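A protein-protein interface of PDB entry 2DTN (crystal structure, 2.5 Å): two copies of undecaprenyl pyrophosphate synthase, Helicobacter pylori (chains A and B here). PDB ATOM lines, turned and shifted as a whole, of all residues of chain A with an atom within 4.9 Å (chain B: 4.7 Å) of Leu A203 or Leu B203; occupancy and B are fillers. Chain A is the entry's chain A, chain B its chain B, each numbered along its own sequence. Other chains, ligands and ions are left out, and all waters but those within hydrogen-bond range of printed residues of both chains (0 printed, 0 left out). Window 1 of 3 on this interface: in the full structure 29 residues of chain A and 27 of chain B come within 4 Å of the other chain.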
ATOM      1  N   SER A 145      11.978   5.664 -30.317  1.00  0.00           N
ATOM      2  CA  SER A 145      13.083   6.552 -30.658  1.00  0.00           C
ATOM      3  C   SER A 145      14.475   5.922 -30.522  1.00  0.00           C
ATOM      4  O   SER A 145      15.293   6.037 -31.429  1.00  0.00           O
ATOM      5  CB  SER A 145      12.982   7.824 -29.815  1.00  0.00           C
ATOM      6  OG  SER A 145      13.688   8.892 -30.409  1.00  0.00           O
ATOM      7  N   LEU A 198       8.146  12.049 -22.314  1.00  0.00           N
ATOM      8  CA  LEU A 198       8.302  12.032 -23.767  1.00  0.00           C
ATOM      9  C   LEU A 198       7.989  10.657 -24.312  1.00  0.00           C
ATOM     10  O   LEU A 198       7.541  10.504 -25.447  1.00  0.00           O
ATOM     11  CB  LEU A 198       9.730  12.402 -24.153  1.00  0.00           C
ATOM     12  CG  LEU A 198      10.153  13.811 -23.764  1.00  0.00           C
ATOM     13  CD1 LEU A 198      11.663  13.897 -23.786  1.00  0.00           C
ATOM     14  CD2 LEU A 198       9.518  14.817 -24.702  1.00  0.00           C
ATOM     15  N   ASN A 200      10.016   8.112 -25.222  1.00  0.00           N
ATOM     16  CA  ASN A 200      10.825   7.598 -26.326  1.00  0.00           C
ATOM     17  C   ASN A 200      10.196   7.880 -27.703  1.00  0.00           C
ATOM     18  O   ASN A 200      10.237   7.044 -28.614  1.00  0.00           O
ATOM     19  CB  ASN A 200      10.989   6.097 -26.064  1.00  0.00           C
ATOM     20  CG  ASN A 200      12.036   5.434 -26.928  1.00  0.00           C
ATOM     21  OD1 ASN A 200      13.097   6.003 -27.221  1.00  0.00           O
ATOM     22  ND2 ASN A 200      11.757   4.188 -27.313  1.00  0.00           N
ATOM     23  N   PHE A 201       9.643   9.080 -27.853  1.00  0.00           N
ATOM     24  CA  PHE A 201       8.989   9.482 -29.089  1.00  0.00           C
ATOM     25  C   PHE A 201       9.642  10.699 -29.751  1.00  0.00           C
ATOM     26  O   PHE A 201       9.666  11.794 -29.187  1.00  0.00           O
ATOM     27  CB  PHE A 201       7.507   9.774 -28.796  1.00  0.00           C
ATOM     28  CG  PHE A 201       6.703  10.196 -29.999  1.00  0.00           C
ATOM     29  CD1 PHE A 201       6.636   9.392 -31.133  1.00  0.00           C
ATOM     30  CD2 PHE A 201       5.976  11.385 -29.981  1.00  0.00           C
ATOM     31  CE1 PHE A 201       5.852   9.771 -32.241  1.00  0.00           C
ATOM     32  CE2 PHE A 201       5.189  11.773 -31.079  1.00  0.00           C
ATOM     33  CZ  PHE A 201       5.128  10.959 -32.213  1.00  0.00           C
ATOM     34  N   LEU A 202      10.175  10.488 -30.951  1.00  0.00           N
ATOM     35  CA  LEU A 202      10.802  11.551 -31.728  1.00  0.00           C
ATOM     36  C   LEU A 202      11.783  12.403 -30.929  1.00  0.00           C
ATOM     37  O   LEU A 202      11.788  13.622 -31.039  1.00  0.00           O
ATOM     38  CB  LEU A 202       9.708  12.442 -32.323  1.00  0.00           C
ATOM     39  CG  LEU A 202       8.691  11.707 -33.199  1.00  0.00           C
ATOM     40  CD1 LEU A 202       7.645  12.681 -33.715  1.00  0.00           C
ATOM     41  CD2 LEU A 202       9.409  11.041 -34.361  1.00  0.00           C
ATOM     42  N   LEU A 203      12.635  11.757 -30.152  1.00  0.00           N
ATOM     43  CA  LEU A 203      13.594  12.468 -29.322  1.00  0.00           C
ATOM     44  C   LEU A 203      14.562  13.334 -30.118  1.00  0.00           C
ATOM     45  O   LEU A 203      14.794  14.498 -29.783  1.00  0.00           O
ATOM     46  CB  LEU A 203      14.359  11.466 -28.464  1.00  0.00           C
ATOM     47  CG  LEU A 203      13.469  10.602 -27.558  1.00  0.00           C
ATOM     48  CD1 LEU A 203      14.331   9.601 -26.803  1.00  0.00           C
ATOM     49  CD2 LEU A 203      12.694  11.496 -26.591  1.00  0.00           C
ATOM     50  N   TRP A 204      15.132  12.762 -31.169  1.00  0.00           N
ATOM     51  CA  TRP A 204      16.066  13.481 -32.023  1.00  0.00           C
ATOM     52  C   TRP A 204      15.327  14.609 -32.746  1.00  0.00           C
ATOM     53  O   TRP A 204      15.725  15.779 -32.684  1.00  0.00           O
ATOM     54  CB  TRP A 204      16.685  12.504 -33.042  1.00  0.00           C
ATOM     55  CG  TRP A 204      17.664  13.131 -34.023  1.00  0.00           C
ATOM     56  CD1 TRP A 204      17.356  13.868 -35.134  1.00  0.00           C
ATOM     57  CD2 TRP A 204      19.096  13.090 -33.961  1.00  0.00           C
ATOM     58  NE1 TRP A 204      18.499  14.287 -35.763  1.00  0.00           N
ATOM     59  CE2 TRP A 204      19.584  13.827 -35.067  1.00  0.00           C
ATOM     60  CE3 TRP A 204      20.016  12.505 -33.078  1.00  0.00           C
ATOM     61  CZ2 TRP A 204      20.956  13.998 -35.314  1.00  0.00           C
ATOM     62  CZ3 TRP A 204      21.383  12.671 -33.323  1.00  0.00           C
ATOM     63  CH2 TRP A 204      21.838  13.413 -34.433  1.00  0.00           C
ATOM     64  N   GLN A 205      14.229  14.243 -33.400  1.00  0.00           N
ATOM     65  CA  GLN A 205      13.433  15.178 -34.184  1.00  0.00           C
ATOM     66  C   GLN A 205      12.685  16.241 -33.385  1.00  0.00           C
ATOM     67  O   GLN A 205      12.133  17.170 -33.970  1.00  0.00           O
ATOM     68  CB  GLN A 205      12.434  14.404 -35.065  1.00  0.00           C
ATOM     69  CG  GLN A 205      13.079  13.299 -35.916  1.00  0.00           C
ATOM     70  CD  GLN A 205      13.080  11.938 -35.224  1.00  0.00           C
ATOM     71  OE1 GLN A 205      13.235  11.843 -34.006  1.00  0.00           O
ATOM     72  NE2 GLN A 205      12.911  10.879 -36.008  1.00  0.00           N
ATOM     73  N   SER A 206      12.673  16.105 -32.058  1.00  0.00           N
ATOM     74  CA  SER A 206      11.976  17.044 -31.185  1.00  0.00           C
ATOM     75  C   SER A 206      12.924  17.780 -30.238  1.00  0.00           C
ATOM     76  O   SER A 206      12.489  18.324 -29.227  1.00  0.00           O
ATOM     77  CB  SER A 206      10.924  16.306 -30.347  1.00  0.00           C
ATOM     78  OG  SER A 206      10.044  15.564 -31.166  1.00  0.00           O
ATOM     79  N   SER A 207      14.211  17.804 -30.563  1.00  0.00           N
ATOM     80  CA  SER A 207      15.186  18.471 -29.708  1.00  0.00           C
ATOM     81  C   SER A 207      14.900  19.963 -29.452  1.00  0.00           C
ATOM     82  O   SER A 207      15.404  20.533 -28.489  1.00  0.00           O
ATOM     83  CB  SER A 207      16.595  18.319 -30.296  1.00  0.00           C
ATOM     84  OG  SER A 207      16.758  19.120 -31.460  1.00  0.00           O
ATOM     85  N   SER B 145      22.998  17.391 -27.367  1.00  0.00           N
ATOM     86  CA  SER B 145      22.514  16.024 -27.378  1.00  0.00           C
ATOM     87  C   SER B 145      22.717  15.351 -28.735  1.00  0.00           C
ATOM     88  O   SER B 145      23.057  14.166 -28.800  1.00  0.00           O
ATOM     89  CB  SER B 145      21.039  16.009 -26.990  1.00  0.00           C
ATOM     90  OG  SER B 145      20.589  14.693 -26.823  1.00  0.00           O
ATOM     91  N   LEU B 198      13.154  21.022 -24.687  1.00  0.00           N
ATOM     92  CA  LEU B 198      14.334  20.382 -24.132  1.00  0.00           C
ATOM     93  C   LEU B 198      15.639  21.012 -24.576  1.00  0.00           C
ATOM     94  O   LEU B 198      16.668  20.841 -23.929  1.00  0.00           O
ATOM     95  CB  LEU B 198      14.317  18.901 -24.501  1.00  0.00           C
ATOM     96  CG  LEU B 198      12.938  18.239 -24.373  1.00  0.00           C
ATOM     97  CD1 LEU B 198      13.021  16.806 -24.863  1.00  0.00           C
ATOM     98  CD2 LEU B 198      12.459  18.287 -22.941  1.00  0.00           C
ATOM     99  N   ASN B 200      17.882  20.397 -27.023  1.00  0.00           N
ATOM    100  CA  ASN B 200      19.006  19.505 -27.321  1.00  0.00           C
ATOM    101  C   ASN B 200      19.748  19.008 -26.090  1.00  0.00           C
ATOM    102  O   ASN B 200      20.952  18.778 -26.138  1.00  0.00           O
ATOM    103  CB  ASN B 200      19.970  20.244 -28.255  1.00  0.00           C
ATOM    104  CG  ASN B 200      20.854  19.318 -29.049  1.00  0.00           C
ATOM    105  OD1 ASN B 200      20.611  18.115 -29.145  1.00  0.00           O
ATOM    106  ND2 ASN B 200      21.887  19.882 -29.649  1.00  0.00           N
ATOM    107  N   PHE B 201      19.024  18.813 -24.994  1.00  0.00           N
ATOM    108  CA  PHE B 201      19.645  18.376 -23.749  1.00  0.00           C
ATOM    109  C   PHE B 201      19.223  16.993 -23.254  1.00  0.00           C
ATOM    110  O   PHE B 201      18.054  16.757 -22.936  1.00  0.00           O
ATOM    111  CB  PHE B 201      19.356  19.419 -22.669  1.00  0.00           C
ATOM    112  CG  PHE B 201      19.957  19.109 -21.322  1.00  0.00           C
ATOM    113  CD1 PHE B 201      21.337  19.002 -21.164  1.00  0.00           C
ATOM    114  CD2 PHE B 201      19.139  19.012 -20.192  1.00  0.00           C
ATOM    115  CE1 PHE B 201      21.893  18.812 -19.908  1.00  0.00           C
ATOM    116  CE2 PHE B 201      19.680  18.823 -18.929  1.00  0.00           C
ATOM    117  CZ  PHE B 201      21.063  18.725 -18.783  1.00  0.00           C
ATOM    118  N   LEU B 202      20.194  16.089 -23.186  1.00  0.00           N
ATOM    119  CA  LEU B 202      19.974  14.737 -22.687  1.00  0.00           C
ATOM    120  C   LEU B 202      18.723  14.089 -23.246  1.00  0.00           C
ATOM    121  O   LEU B 202      17.957  13.471 -22.504  1.00  0.00           O
ATOM    122  CB  LEU B 202      19.882  14.754 -21.154  1.00  0.00           C
ATOM    123  CG  LEU B 202      21.104  15.227 -20.361  1.00  0.00           C
ATOM    124  CD1 LEU B 202      20.777  15.204 -18.866  1.00  0.00           C
ATOM    125  CD2 LEU B 202      22.291  14.340 -20.668  1.00  0.00           C
ATOM    126  N   LEU B 203      18.533  14.211 -24.554  1.00  0.00           N
ATOM    127  CA  LEU B 203      17.357  13.654 -25.208  1.00  0.00           C
ATOM    128  C   LEU B 203      17.265  12.129 -25.048  1.00  0.00           C
ATOM    129  O   LEU B 203      16.227  11.600 -24.670  1.00  0.00           O
ATOM    130  CB  LEU B 203      17.372  14.042 -26.694  1.00  0.00           C
ATOM    131  CG  LEU B 203      17.624  15.535 -26.986  1.00  0.00           C
ATOM    132  CD1 LEU B 203      17.924  15.721 -28.463  1.00  0.00           C
ATOM    133  CD2 LEU B 203      16.421  16.375 -26.562  1.00  0.00           C
ATOM    134  N   TRP B 204      18.355  11.431 -25.334  1.00  0.00           N
ATOM    135  CA  TRP B 204      18.380   9.981 -25.227  1.00  0.00           C
ATOM    136  C   TRP B 204      18.227   9.536 -23.769  1.00  0.00           C
ATOM    137  O   TRP B 204      17.428   8.650 -23.453  1.00  0.00           O
ATOM    138  CB  TRP B 204      19.698   9.470 -25.835  1.00  0.00           C
ATOM    139  CG  TRP B 204      19.982   8.004 -25.649  1.00  0.00           C
ATOM    140  CD1 TRP B 204      20.320   7.381 -24.489  1.00  0.00           C
ATOM    141  CD2 TRP B 204      19.967   6.978 -26.666  1.00  0.00           C
ATOM    142  NE1 TRP B 204      20.520   6.038 -24.709  1.00  0.00           N
ATOM    143  CE2 TRP B 204      20.311   5.762 -26.035  1.00  0.00           C
ATOM    144  CE3 TRP B 204      19.698   6.973 -28.045  1.00  0.00           C
ATOM    145  CZ2 TRP B 204      20.392   4.546 -26.730  1.00  0.00           C
ATOM    146  CZ3 TRP B 204      19.777   5.765 -28.741  1.00  0.00           C
ATOM    147  CH2 TRP B 204      20.122   4.565 -28.076  1.00  0.00           C
ATOM    148  N   GLN B 205      18.983  10.175 -22.883  1.00  0.00           N
ATOM    149  CA  GLN B 205      18.971   9.848 -21.461  1.00  0.00           C
ATOM    150  C   GLN B 205      17.682  10.229 -20.724  1.00  0.00           C
ATOM    151  O   GLN B 205      17.438   9.753 -19.610  1.00  0.00           O
ATOM    152  CB  GLN B 205      20.181  10.506 -20.780  1.00  0.00           C
ATOM    153  CG  GLN B 205      21.514  10.120 -21.412  1.00  0.00           C
ATOM    154  CD  GLN B 205      22.017  11.109 -22.469  1.00  0.00           C
ATOM    155  OE1 GLN B 205      21.242  11.747 -23.198  1.00  0.00           O
ATOM    156  NE2 GLN B 205      23.334  11.222 -22.566  1.00  0.00           N
ATOM    157  N   SER B 206      16.859  11.074 -21.345  1.00  0.00           N
ATOM    158  CA  SER B 206      15.599  11.522 -20.741  1.00  0.00           C
ATOM    159  C   SER B 206      14.338  11.005 -21.411  1.00  0.00           C
ATOM    160  O   SER B 206      13.270  11.553 -21.185  1.00  0.00           O
ATOM    161  CB  SER B 206      15.523  13.049 -20.731  1.00  0.00           C
ATOM    162  OG  SER B 206      16.561  13.595 -19.949  1.00  0.00           O
ATOM    163  N   SER B 207      14.459   9.951 -22.211  1.00  0.00           N
ATOM    164  CA  SER B 207      13.321   9.380 -22.931  1.00  0.00           C
ATOM    165  C   SER B 207      12.075   9.047 -22.093  1.00  0.00           C
ATOM    166  O   SER B 207      10.953   9.107 -22.595  1.00  0.00           O
ATOM    167  CB  SER B 207      13.762   8.126 -23.680  1.00  0.00           C
ATOM    168  OG  SER B 207      14.049   7.084 -22.769  1.00  0.00           O
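O of Asn A200 lies within hydrogen-bond range of N of Ser A145 (2.8 Å).
The backbone NH of Leu A203 is in hydrogen-bond range of the side-chain hydroxyl of Ser A145 (3.1 Å).
The backbone carbonyl oxygen (O) of Asn B200 is in hydrogen-bond range of the backbone NH (N) of Ser B145.
The side-chain hydroxyl (OG) of Ser B145 lies close to the backbone NH (N) of Leu B203.
The backbone carbonyl oxygen of Leu B202 is in hydrogen-bond range of the side-chain hydroxyl of Ser B206, 2.9 Å away.
The backbone NH of Asn A200 is in hydrogen-bond range of the backbone carbonyl oxygen of Ser B207, at 3.0 Å.
The backbone carbonyl oxygen (O) of Ser A207 sits at hydrogen-bond distance from the backbone NH (N) of Asn B200, at 2.9 Å.
Leu A198 touches its own counterpart, Leu B198.
Leu A198 touches Ser B206, but with the chains exchanged Ser A206 does not touch Leu B198 (4.7 Å).
Asn A200 touches Ser B207, and with the chains exchanged Ser A207 touches Asn B200.
Leu A203 touches Ser B207, and with the chains exchanged Ser A207 touches Leu B203.
10 positions are printed for both chains.
Of the 9 pairs that touch across the chains among the printed residues, 8 have their exchanged pair printed and touching as well.
CD1 of Leu B198 touches CD1 of Leu A198, at 3.4 Å.
O of Ser B206 touches CD1 of Leu A198, at 3.9 Å.
Leu A198 touches Ser B207.
Leu A203 touches Leu B203.
CB of Ser B207 touches CD1 of Leu A203, 3.5 Å away.
Ser A207 touches Leu B198.
Ser A207 touches Leu B203.
Ser A145 touches none of the printed residues of chain B.
Of the printed residues of chain B, Asn A200 touches Ser B207.
Leu A202 touches none of the printed residues of chain B.
Of the printed residues of chain B, Ser A207 touches Leu B198 (3.9 Å), Asn B200 (2.9 Å) and Leu B203 (3.4 Å).
The nearest residue of chain B that does not touch Leu A203 is Trp B204 (4.4 Å).
Of the 10 printed residues of chain A, 4 touch a printed residue of chain B.
Along chain A the printed residues that touch a printed residue of chain B span positions 198 to 207.
Hydrophobic or aromatic side chains of chain B within 4 Å of the printed part of chain A: Leu B198 and Leu B203.
Along chain B the printed residues that touch a printed residue of chain A span positions 198 to 207.
Among the printed residues, no Asp or Glu carboxylate lies within 4 Å of a Lys or Arg side-chain nitrogen of the other chain.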
